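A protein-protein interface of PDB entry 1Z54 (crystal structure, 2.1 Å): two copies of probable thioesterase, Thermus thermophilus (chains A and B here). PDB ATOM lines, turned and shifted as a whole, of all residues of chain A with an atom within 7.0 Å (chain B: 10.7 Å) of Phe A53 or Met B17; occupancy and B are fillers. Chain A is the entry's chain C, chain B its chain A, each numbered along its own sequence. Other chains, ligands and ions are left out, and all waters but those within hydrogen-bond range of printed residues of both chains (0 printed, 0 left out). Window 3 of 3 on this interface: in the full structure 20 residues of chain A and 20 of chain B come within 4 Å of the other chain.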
ATOM      1  N   TYR A  44      -4.824  20.023  12.581  1.00  0.00           N
ATOM      2  CA  TYR A  44      -3.396  20.225  12.821  1.00  0.00           C
ATOM      3  C   TYR A  44      -2.735  19.316  13.838  1.00  0.00           C
ATOM      4  O   TYR A  44      -1.606  18.878  13.620  1.00  0.00           O
ATOM      5  CB  TYR A  44      -3.102  21.687  13.173  1.00  0.00           C
ATOM      6  CG  TYR A  44      -1.631  22.034  13.039  1.00  0.00           C
ATOM      7  CD1 TYR A  44      -0.944  21.778  11.850  1.00  0.00           C
ATOM      8  CD2 TYR A  44      -0.919  22.579  14.105  1.00  0.00           C
ATOM      9  CE1 TYR A  44       0.419  22.049  11.732  1.00  0.00           C
ATOM     10  CE2 TYR A  44       0.443  22.857  13.995  1.00  0.00           C
ATOM     11  CZ  TYR A  44       1.105  22.583  12.810  1.00  0.00           C
ATOM     12  OH  TYR A  44       2.461  22.784  12.726  1.00  0.00           O
ATOM     13  N   VAL A  47      -1.910  16.295  12.138  1.00  0.00           N
ATOM     14  CA  VAL A  47      -0.797  16.528  11.220  1.00  0.00           C
ATOM     15  C   VAL A  47       0.529  16.393  11.968  1.00  0.00           C
ATOM     16  O   VAL A  47       1.421  15.642  11.543  1.00  0.00           O
ATOM     17  CB  VAL A  47      -0.875  17.938  10.597  1.00  0.00           C
ATOM     18  CG1 VAL A  47       0.424  18.255   9.840  1.00  0.00           C
ATOM     19  CG2 VAL A  47      -2.076  18.019   9.658  1.00  0.00           C
ATOM     20  N   GLU A  48       0.657  17.111  13.083  1.00  0.00           N
ATOM     21  CA  GLU A  48       1.886  17.055  13.870  1.00  0.00           C
ATOM     22  C   GLU A  48       2.127  15.646  14.394  1.00  0.00           C
ATOM     23  O   GLU A  48       3.264  15.195  14.486  1.00  0.00           O
ATOM     24  CB  GLU A  48       1.839  18.044  15.041  1.00  0.00           C
ATOM     25  CG  GLU A  48       1.872  19.518  14.636  1.00  0.00           C
ATOM     26  CD  GLU A  48       2.570  20.397  15.675  1.00  0.00           C
ATOM     27  OE1 GLU A  48       2.477  20.089  16.883  1.00  0.00           O
ATOM     28  OE2 GLU A  48       3.205  21.401  15.286  1.00  0.00           O
ATOM     29  N   ALA A  49       1.051  14.947  14.727  1.00  0.00           N
ATOM     30  CA  ALA A  49       1.173  13.585  15.228  1.00  0.00           C
ATOM     31  C   ALA A  49       1.825  12.687  14.174  1.00  0.00           C
ATOM     32  O   ALA A  49       2.474  11.699  14.508  1.00  0.00           O
ATOM     33  CB  ALA A  49      -0.206  13.038  15.614  1.00  0.00           C
ATOM     34  N   ARG A  50       1.643  13.036  12.903  1.00  0.00           N
ATOM     35  CA  ARG A  50       2.225  12.269  11.804  1.00  0.00           C
ATOM     36  C   ARG A  50       3.658  12.713  11.548  1.00  0.00           C
ATOM     37  O   ARG A  50       4.315  12.219  10.629  1.00  0.00           O
ATOM     38  CB  ARG A  50       1.392  12.441  10.529  1.00  0.00           C
ATOM     39  CG  ARG A  50       0.048  11.720  10.569  1.00  0.00           C
ATOM     40  CD  ARG A  50      -0.840  12.129   9.407  1.00  0.00           C
ATOM     41  NE  ARG A  50      -0.213  11.864   8.120  1.00  0.00           N
ATOM     42  CZ  ARG A  50      -0.648  12.346   6.959  1.00  0.00           C
ATOM     43  NH1 ARG A  50      -0.008  12.047   5.838  1.00  0.00           N
ATOM     44  NH2 ARG A  50      -1.721  13.129   6.917  1.00  0.00           N
ATOM     45  N   GLY A  51       4.137  13.645  12.368  1.00  0.00           N
ATOM     46  CA  GLY A  51       5.492  14.142  12.218  1.00  0.00           C
ATOM     47  C   GLY A  51       5.600  15.203  11.140  1.00  0.00           C
ATOM     48  O   GLY A  51       6.615  15.305  10.456  1.00  0.00           O
ATOM     49  N   VAL A  52       4.546  15.998  10.990  1.00  0.00           N
ATOM     50  CA  VAL A  52       4.504  17.059   9.988  1.00  0.00           C
ATOM     51  C   VAL A  52       4.184  18.374  10.700  1.00  0.00           C
ATOM     52  O   VAL A  52       3.262  18.436  11.512  1.00  0.00           O
ATOM     53  CB  VAL A  52       3.424  16.756   8.916  1.00  0.00           C
ATOM     54  CG1 VAL A  52       3.403  17.844   7.857  1.00  0.00           C
ATOM     55  CG2 VAL A  52       3.705  15.408   8.275  1.00  0.00           C
ATOM     56  N   PHE A  53       4.943  19.418  10.380  1.00  0.00           N
ATOM     57  CA  PHE A  53       4.787  20.724  11.014  1.00  0.00           C
ATOM     58  C   PHE A  53       4.795  21.868  10.007  1.00  0.00           C
ATOM     59  O   PHE A  53       5.384  21.754   8.928  1.00  0.00           O
ATOM     60  CB  PHE A  53       5.926  20.924  12.012  1.00  0.00           C
ATOM     61  CG  PHE A  53       6.066  19.796  12.994  1.00  0.00           C
ATOM     62  CD1 PHE A  53       5.342  19.794  14.181  1.00  0.00           C
ATOM     63  CD2 PHE A  53       6.877  18.703  12.701  1.00  0.00           C
ATOM     64  CE1 PHE A  53       5.416  18.718  15.067  1.00  0.00           C
ATOM     65  CE2 PHE A  53       6.961  17.620  13.575  1.00  0.00           C
ATOM     66  CZ  PHE A  53       6.226  17.627  14.763  1.00  0.00           C
ATOM     67  N   PHE A  54       4.140  22.970  10.378  1.00  0.00           N
ATOM     68  CA  PHE A  54       4.066  24.164   9.541  1.00  0.00           C
ATOM     69  C   PHE A  54       4.589  25.390  10.293  1.00  0.00           C
ATOM     70  O   PHE A  54       3.852  26.347  10.534  1.00  0.00           O
ATOM     71  CB  PHE A  54       2.623  24.412   9.091  1.00  0.00           C
ATOM     72  CG  PHE A  54       2.122  23.413   8.090  1.00  0.00           C
ATOM     73  CD1 PHE A  54       0.774  23.099   8.024  1.00  0.00           C
ATOM     74  CD2 PHE A  54       2.999  22.787   7.213  1.00  0.00           C
ATOM     75  CE1 PHE A  54       0.305  22.173   7.102  1.00  0.00           C
ATOM     76  CE2 PHE A  54       2.539  21.861   6.287  1.00  0.00           C
ATOM     77  CZ  PHE A  54       1.189  21.553   6.230  1.00  0.00           C
ATOM     78  N   PRO A  55       5.879  25.374  10.672  1.00  0.00           N
ATOM     79  CA  PRO A  55       6.484  26.499  11.395  1.00  0.00           C
ATOM     80  C   PRO A  55       6.324  27.815  10.637  1.00  0.00           C
ATOM     81  O   PRO A  55       6.292  27.827   9.411  1.00  0.00           O
ATOM     82  CB  PRO A  55       7.950  26.072  11.535  1.00  0.00           C
ATOM     83  CG  PRO A  55       8.168  25.206  10.332  1.00  0.00           C
ATOM     84  CD  PRO A  55       6.899  24.383  10.288  1.00  0.00           C
ATOM     85  N   VAL A  56       6.198  28.915  11.375  1.00  0.00           N
ATOM     86  CA  VAL A  56       6.047  30.239  10.779  1.00  0.00           C
ATOM     87  C   VAL A  56       7.426  30.829  10.493  1.00  0.00           C
ATOM     88  O   VAL A  56       8.278  30.859  11.377  1.00  0.00           O
ATOM     89  CB  VAL A  56       5.294  31.218  11.723  1.00  0.00           C
ATOM     90  CG1 VAL A  56       5.294  32.619  11.129  1.00  0.00           C
ATOM     91  CG2 VAL A  56       3.865  30.748  11.948  1.00  0.00           C
ATOM     92  N   LEU A  87       3.675  27.621   2.323  1.00  0.00           N
ATOM     93  CA  LEU A  87       2.283  28.062   2.366  1.00  0.00           C
ATOM     94  C   LEU A  87       2.236  29.527   2.766  1.00  0.00           C
ATOM     95  O   LEU A  87       3.095  30.005   3.506  1.00  0.00           O
ATOM     96  CB  LEU A  87       1.481  27.289   3.425  1.00  0.00           C
ATOM     97  CG  LEU A  87       1.415  25.765   3.498  1.00  0.00           C
ATOM     98  CD1 LEU A  87       0.863  25.236   2.205  1.00  0.00           C
ATOM     99  CD2 LEU A  87       2.798  25.184   3.778  1.00  0.00           C
ATOM    100  N   HIS A 107       4.684  30.047   5.780  1.00  0.00           N
ATOM    101  CA  HIS A 107       5.150  28.835   6.439  1.00  0.00           C
ATOM    102  C   HIS A 107       5.994  27.938   5.556  1.00  0.00           C
ATOM    103  O   HIS A 107       5.862  27.946   4.332  1.00  0.00           O
ATOM    104  CB  HIS A 107       3.965  27.985   6.926  1.00  0.00           C
ATOM    105  CG  HIS A 107       3.009  28.702   7.829  1.00  0.00           C
ATOM    106  ND1 HIS A 107       2.156  29.691   7.383  1.00  0.00           N
ATOM    107  CD2 HIS A 107       2.733  28.534   9.143  1.00  0.00           C
ATOM    108  CE1 HIS A 107       1.393  30.097   8.383  1.00  0.00           C
ATOM    109  NE2 HIS A 107       1.722  29.410   9.462  1.00  0.00           N
ATOM    110  N   LEU A 108       6.851  27.159   6.203  1.00  0.00           N
ATOM    111  CA  LEU A 108       7.679  26.169   5.526  1.00  0.00           C
ATOM    112  C   LEU A 108       7.143  24.868   6.095  1.00  0.00           C
ATOM    113  O   LEU A 108       6.391  24.892   7.069  1.00  0.00           O
ATOM    114  CB  LEU A 108       9.157  26.311   5.910  1.00  0.00           C
ATOM    115  CG  LEU A 108       9.959  27.427   5.242  1.00  0.00           C
ATOM    116  CD1 LEU A 108      11.402  27.345   5.712  1.00  0.00           C
ATOM    117  CD2 LEU A 108       9.885  27.296   3.724  1.00  0.00           C
ATOM    118  N   CYS A 109       7.505  23.740   5.504  1.00  0.00           N
ATOM    119  CA  CYS A 109       7.036  22.470   6.028  1.00  0.00           C
ATOM    120  C   CYS A 109       8.189  21.678   6.625  1.00  0.00           C
ATOM    121  O   CYS A 109       9.250  21.549   6.017  1.00  0.00           O
ATOM    122  CB  CYS A 109       6.363  21.640   4.941  1.00  0.00           C
ATOM    123  SG  CYS A 109       5.726  20.072   5.593  1.00  0.00           S
ATOM    124  N   GLN A 110       7.974  21.157   7.824  1.00  0.00           N
ATOM    125  CA  GLN A 110       8.996  20.383   8.507  1.00  0.00           C
ATOM    126  C   GLN A 110       8.510  18.966   8.777  1.00  0.00           C
ATOM    127  O   GLN A 110       7.488  18.763   9.436  1.00  0.00           O
ATOM    128  CB  GLN A 110       9.376  21.059   9.831  1.00  0.00           C
ATOM    129  CG  GLN A 110      10.466  20.330  10.606  1.00  0.00           C
ATOM    130  CD  GLN A 110      10.782  20.985  11.940  1.00  0.00           C
ATOM    131  OE1 GLN A 110      11.082  22.178  12.005  1.00  0.00           O
ATOM    132  NE2 GLN A 110      10.720  20.205  13.012  1.00  0.00           N
ATOM    133  N   VAL A 111       9.241  17.992   8.245  1.00  0.00           N
ATOM    134  CA  VAL A 111       8.921  16.584   8.457  1.00  0.00           C
ATOM    135  C   VAL A 111      10.059  16.090   9.331  1.00  0.00           C
ATOM    136  O   VAL A 111      11.230  16.159   8.945  1.00  0.00           O
ATOM    137  CB  VAL A 111       8.898  15.784   7.129  1.00  0.00           C
ATOM    138  CG1 VAL A 111       8.629  14.309   7.415  1.00  0.00           C
ATOM    139  CG2 VAL A 111       7.832  16.339   6.198  1.00  0.00           C
ATOM    140  N   GLY A 112       9.723  15.599  10.517  1.00  0.00           N
ATOM    141  CA  GLY A 112      10.765  15.156  11.420  1.00  0.00           C
ATOM    142  C   GLY A 112      11.467  16.387  11.978  1.00  0.00           C
ATOM    143  O   GLY A 112      10.878  17.131  12.761  1.00  0.00           O
ATOM    144  N   GLU A 113      12.705  16.631  11.559  1.00  0.00           N
ATOM    145  CA  GLU A 113      13.449  17.783  12.060  1.00  0.00           C
ATOM    146  C   GLU A 113      14.079  18.654  10.969  1.00  0.00           C
ATOM    147  O   GLU A 113      14.980  19.448  11.251  1.00  0.00           O
ATOM    148  CB  GLU A 113      14.546  17.310  13.018  1.00  0.00           C
ATOM    149  CG  GLU A 113      14.031  16.508  14.209  1.00  0.00           C
ATOM    150  CD  GLU A 113      13.238  17.352  15.191  1.00  0.00           C
ATOM    151  OE1 GLU A 113      12.660  16.778  16.139  1.00  0.00           O
ATOM    152  OE2 GLU A 113      13.198  18.590  15.023  1.00  0.00           O
ATOM    153  N   TYR B  11      10.171  30.259  30.239  1.00  0.00           N
ATOM    154  CA  TYR B  11       9.615  28.940  29.954  1.00  0.00           C
ATOM    155  C   TYR B  11       8.227  29.047  29.321  1.00  0.00           C
ATOM    156  O   TYR B  11       7.934  28.386  28.324  1.00  0.00           O
ATOM    157  CB  TYR B  11       9.525  28.124  31.246  1.00  0.00           C
ATOM    158  CG  TYR B  11       9.364  26.640  31.023  1.00  0.00           C
ATOM    159  CD1 TYR B  11      10.465  25.845  30.702  1.00  0.00           C
ATOM    160  CD2 TYR B  11       8.108  26.033  31.095  1.00  0.00           C
ATOM    161  CE1 TYR B  11      10.325  24.485  30.456  1.00  0.00           C
ATOM    162  CE2 TYR B  11       7.954  24.668  30.847  1.00  0.00           C
ATOM    163  CZ  TYR B  11       9.068  23.903  30.527  1.00  0.00           C
ATOM    164  OH  TYR B  11       8.923  22.560  30.256  1.00  0.00           O
ATOM    165  N   GLU B  13       7.035  31.100  27.443  1.00  0.00           N
ATOM    166  CA  GLU B  13       7.065  31.575  26.064  1.00  0.00           C
ATOM    167  C   GLU B  13       7.409  30.510  25.008  1.00  0.00           C
ATOM    168  O   GLU B  13       7.309  30.765  23.814  1.00  0.00           O
ATOM    169  CB  GLU B  13       8.025  32.777  25.978  1.00  0.00           C
ATOM    170  CG  GLU B  13       7.745  33.808  27.083  1.00  0.00           C
ATOM    171  CD  GLU B  13       8.759  34.941  27.149  1.00  0.00           C
ATOM    172  OE1 GLU B  13       9.967  34.672  27.030  1.00  0.00           O
ATOM    173  OE2 GLU B  13       8.342  36.103  27.345  1.00  0.00           O
ATOM    174  N   THR B  14       7.801  29.316  25.441  1.00  0.00           N
ATOM    175  CA  THR B  14       8.131  28.240  24.503  1.00  0.00           C
ATOM    176  C   THR B  14       6.854  27.515  24.038  1.00  0.00           C
ATOM    177  O   THR B  14       5.872  27.452  24.784  1.00  0.00           O
ATOM    178  CB  THR B  14       9.051  27.190  25.162  1.00  0.00           C
ATOM    179  OG1 THR B  14       8.341  26.538  26.224  1.00  0.00           O
ATOM    180  CG2 THR B  14      10.302  27.849  25.721  1.00  0.00           C
ATOM    181  N   ASP B  15       6.865  26.978  22.818  1.00  0.00           N
ATOM    182  CA  ASP B  15       5.708  26.240  22.298  1.00  0.00           C
ATOM    183  C   ASP B  15       5.987  24.732  22.326  1.00  0.00           C
ATOM    184  O   ASP B  15       6.984  24.288  22.905  1.00  0.00           O
ATOM    185  CB  ASP B  15       5.365  26.676  20.861  1.00  0.00           C
ATOM    186  CG  ASP B  15       6.435  26.289  19.847  1.00  0.00           C
ATOM    187  OD1 ASP B  15       7.306  25.443  20.165  1.00  0.00           O
ATOM    188  OD2 ASP B  15       6.394  26.829  18.717  1.00  0.00           O
ATOM    189  N   GLN B  16       5.113  23.953  21.685  1.00  0.00           N
ATOM    190  CA  GLN B  16       5.258  22.497  21.646  1.00  0.00           C
ATOM    191  C   GLN B  16       6.456  22.030  20.835  1.00  0.00           C
ATOM    192  O   GLN B  16       7.015  20.967  21.108  1.00  0.00           O
ATOM    193  CB  GLN B  16       4.004  21.829  21.067  1.00  0.00           C
ATOM    194  CG  GLN B  16       2.797  21.849  21.964  1.00  0.00           C
ATOM    195  CD  GLN B  16       1.692  20.932  21.472  1.00  0.00           C
ATOM    196  OE1 GLN B  16       1.417  20.859  20.272  1.00  0.00           O
ATOM    197  NE2 GLN B  16       1.047  20.231  22.402  1.00  0.00           N
ATOM    198  N   MET B  17       6.830  22.806  19.822  1.00  0.00           N
ATOM    199  CA  MET B  17       7.967  22.457  18.980  1.00  0.00           C
ATOM    200  C   MET B  17       9.276  22.744  19.736  1.00  0.00           C
ATOM    201  O   MET B  17      10.373  22.513  19.219  1.00  0.00           O
ATOM    202  CB  MET B  17       7.904  23.229  17.638  1.00  0.00           C
ATOM    203  CG  MET B  17       6.889  22.651  16.588  1.00  0.00           C
ATOM    204  SD  MET B  17       6.809  23.567  14.967  1.00  0.00           S
ATOM    205  CE  MET B  17       8.129  22.737  13.997  1.00  0.00           C
ATOM    206  N   GLY B  18       9.148  23.248  20.964  1.00  0.00           N
ATOM    207  CA  GLY B  18      10.314  23.530  21.789  1.00  0.00           C
ATOM    208  C   GLY B  18      11.070  24.818  21.503  1.00  0.00           C
ATOM    209  O   GLY B  18      12.265  24.913  21.791  1.00  0.00           O
ATOM    210  N   VAL B  19      10.388  25.808  20.940  1.00  0.00           N
ATOM    211  CA  VAL B  19      11.013  27.090  20.642  1.00  0.00           C
ATOM    212  C   VAL B  19      10.099  28.223  21.114  1.00  0.00           C
ATOM    213  O   VAL B  19       8.947  27.980  21.487  1.00  0.00           O
ATOM    214  CB  VAL B  19      11.278  27.237  19.132  1.00  0.00           C
ATOM    215  CG1 VAL B  19      12.250  26.152  18.669  1.00  0.00           C
ATOM    216  CG2 VAL B  19       9.971  27.150  18.359  1.00  0.00           C
ATOM    217  N   VAL B  20      10.613  29.451  21.129  1.00  0.00           N
ATOM    218  CA  VAL B  20       9.795  30.587  21.545  1.00  0.00           C
ATOM    219  C   VAL B  20       8.691  30.714  20.506  1.00  0.00           C
ATOM    220  O   VAL B  20       8.967  30.740  19.304  1.00  0.00           O
ATOM    221  CB  VAL B  20      10.608  31.898  21.579  1.00  0.00           C
ATOM    222  CG1 VAL B  20       9.674  33.083  21.792  1.00  0.00           C
ATOM    223  CG2 VAL B  20      11.660  31.832  22.691  1.00  0.00           C
ATOM    224  N   HIS B  21       7.445  30.786  20.957  1.00  0.00           N
ATOM    225  CA  HIS B  21       6.332  30.890  20.023  1.00  0.00           C
ATOM    226  C   HIS B  21       6.429  32.185  19.224  1.00  0.00           C
ATOM    227  O   HIS B  21       6.730  33.245  19.772  1.00  0.00           O
ATOM    228  CB  HIS B  21       5.002  30.818  20.768  1.00  0.00           C
ATOM    229  CG  HIS B  21       3.822  30.658  19.863  1.00  0.00           C
ATOM    230  ND1 HIS B  21       3.033  31.717  19.470  1.00  0.00           N
ATOM    231  CD2 HIS B  21       3.306  29.559  19.262  1.00  0.00           C
ATOM    232  CE1 HIS B  21       2.075  31.276  18.672  1.00  0.00           C
ATOM    233  NE2 HIS B  21       2.218  29.970  18.530  1.00  0.00           N
ATOM    234  N   HIS B  22       6.161  32.100  17.927  1.00  0.00           N
ATOM    235  CA  HIS B  22       6.272  33.267  17.069  1.00  0.00           C
ATOM    236  C   HIS B  22       5.492  34.505  17.513  1.00  0.00           C
ATOM    237  O   HIS B  22       5.874  35.628  17.165  1.00  0.00           O
ATOM    238  CB  HIS B  22       5.915  32.893  15.626  1.00  0.00           C
ATOM    239  CG  HIS B  22       4.502  32.440  15.444  1.00  0.00           C
ATOM    240  ND1 HIS B  22       3.493  33.292  15.052  1.00  0.00           N
ATOM    241  CD2 HIS B  22       3.930  31.221  15.592  1.00  0.00           C
ATOM    242  CE1 HIS B  22       2.361  32.617  14.960  1.00  0.00           C
ATOM    243  NE2 HIS B  22       2.600  31.359  15.282  1.00  0.00           N
ATOM    244  N   PRO B  66      15.452  29.881  15.613  1.00  0.00           N
ATOM    245  CA  PRO B  66      14.719  29.965  16.874  1.00  0.00           C
ATOM    246  C   PRO B  66      15.497  30.325  18.124  1.00  0.00           C
ATOM    247  O   PRO B  66      16.718  30.184  18.187  1.00  0.00           O
ATOM    248  CB  PRO B  66      14.091  28.582  16.985  1.00  0.00           C
ATOM    249  CG  PRO B  66      15.191  27.706  16.450  1.00  0.00           C
ATOM    250  CD  PRO B  66      15.693  28.476  15.230  1.00  0.00           C
ATOM    251  N   ALA B  67      14.752  30.805  19.114  1.00  0.00           N
ATOM    252  CA  ALA B  67      15.295  31.148  20.415  1.00  0.00           C
ATOM    253  C   ALA B  67      14.751  30.023  21.291  1.00  0.00           C
ATOM    254  O   ALA B  67      13.695  29.462  20.996  1.00  0.00           O
ATOM    255  CB  ALA B  67      14.755  32.498  20.880  1.00  0.00           C
ATOM    256  N   ARG B  68      15.463  29.678  22.354  1.00  0.00           N
ATOM    257  CA  ARG B  68      15.009  28.598  23.226  1.00  0.00           C
ATOM    258  C   ARG B  68      15.109  28.930  24.708  1.00  0.00           C
ATOM    259  O   ARG B  68      15.873  29.818  25.111  1.00  0.00           O
ATOM    260  CB  ARG B  68      15.823  27.329  22.966  1.00  0.00           C
ATOM    261  CG  ARG B  68      15.661  26.734  21.587  1.00  0.00           C
ATOM    262  CD  ARG B  68      16.178  25.302  21.554  1.00  0.00           C
ATOM    263  NE  ARG B  68      15.944  24.673  20.256  1.00  0.00           N
ATOM    264  CZ  ARG B  68      16.629  24.958  19.151  1.00  0.00           C
ATOM    265  NH1 ARG B  68      17.602  25.859  19.180  1.00  0.00           N
ATOM    266  NH2 ARG B  68      16.332  24.349  18.012  1.00  0.00           N
ATOM    267  N   PHE B  69      14.331  28.211  25.515  1.00  0.00           N
ATOM    268  CA  PHE B  69      14.377  28.398  26.954  1.00  0.00           C
ATOM    269  C   PHE B  69      15.781  27.991  27.378  1.00  0.00           C
ATOM    270  O   PHE B  69      16.287  26.947  26.961  1.00  0.00           O
ATOM    271  CB  PHE B  69      13.361  27.509  27.662  1.00  0.00           C
ATOM    272  CG  PHE B  69      13.491  27.534  29.158  1.00  0.00           C
ATOM    273  CD1 PHE B  69      13.898  26.400  29.855  1.00  0.00           C
ATOM    274  CD2 PHE B  69      13.237  28.709  29.869  1.00  0.00           C
ATOM    275  CE1 PHE B  69      14.049  26.434  31.245  1.00  0.00           C
ATOM    276  CE2 PHE B  69      13.388  28.757  31.253  1.00  0.00           C
ATOM    277  CZ  PHE B  69      13.795  27.618  31.946  1.00  0.00           C
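The backbone NH of Phe A53 sits at hydrogen-bond distance from the backbone carbonyl oxygen of Gln A110, at 2.8 Å.
The side-chain carboxylate of Asp B15 lies within hydrogen-bond range of the backbone NH of Met B17 (2.7 Å).
O of Phe A53 lies close to SG of Cys A109 (3.8 Å).
OE2 of Glu A48 is in hydrogen-bond range of OH of Tyr A44, 3.0 Å away.
O of Gly A112 sits at hydrogen-bond distance from NE2 of Gln A110, 3.1 Å away.
Among the printed residues, merely in contact across the chains: Glu A48 with Gln B16 (3.6 Å), Phe A53 with Met B17 (3.5 Å), Val A56 with His B22 (3.6 Å) and Gln A110 with Met B17 (3.6 Å).
Phe A53 touches just one residue of chain B: Met B17 (3.5 Å).
Of the printed residues of chain B, Glu A48 touches Gln B16.
No residue of chain B comes within 4 Å of Val A52.
No residue of chain B comes within 4 Å of Phe A54.
Gln A110 touches one residue of chain B.
No residue of chain B comes within 4 Å of Gly A112.
Of the printed residues of chain A, Gln B16 touches Glu A48 (3.6 Å).
Printed residues of chain B within 4 Å of Val A56: His B22.
Printed residues of chain A within 4 Å of His B22: Val A56.
Val A111 touches none of the printed residues of chain B.
Val B19 touches none of the printed residues of chain A.
The nearest printed residue of chain A that does not touch His B22 is His A107 (6.2 Å).
Of the 15 printed residues of chain B, 3 touch a printed residue of chain A.
Hydrophobic or aromatic side chains of chain B within 4 Å of the printed part of chain A: Met B17 and His B22.
No position is printed for both chains.
Of the 4 pairs that touch across the chains among the printed residues, none has its exchanged pair printed and touching as well.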
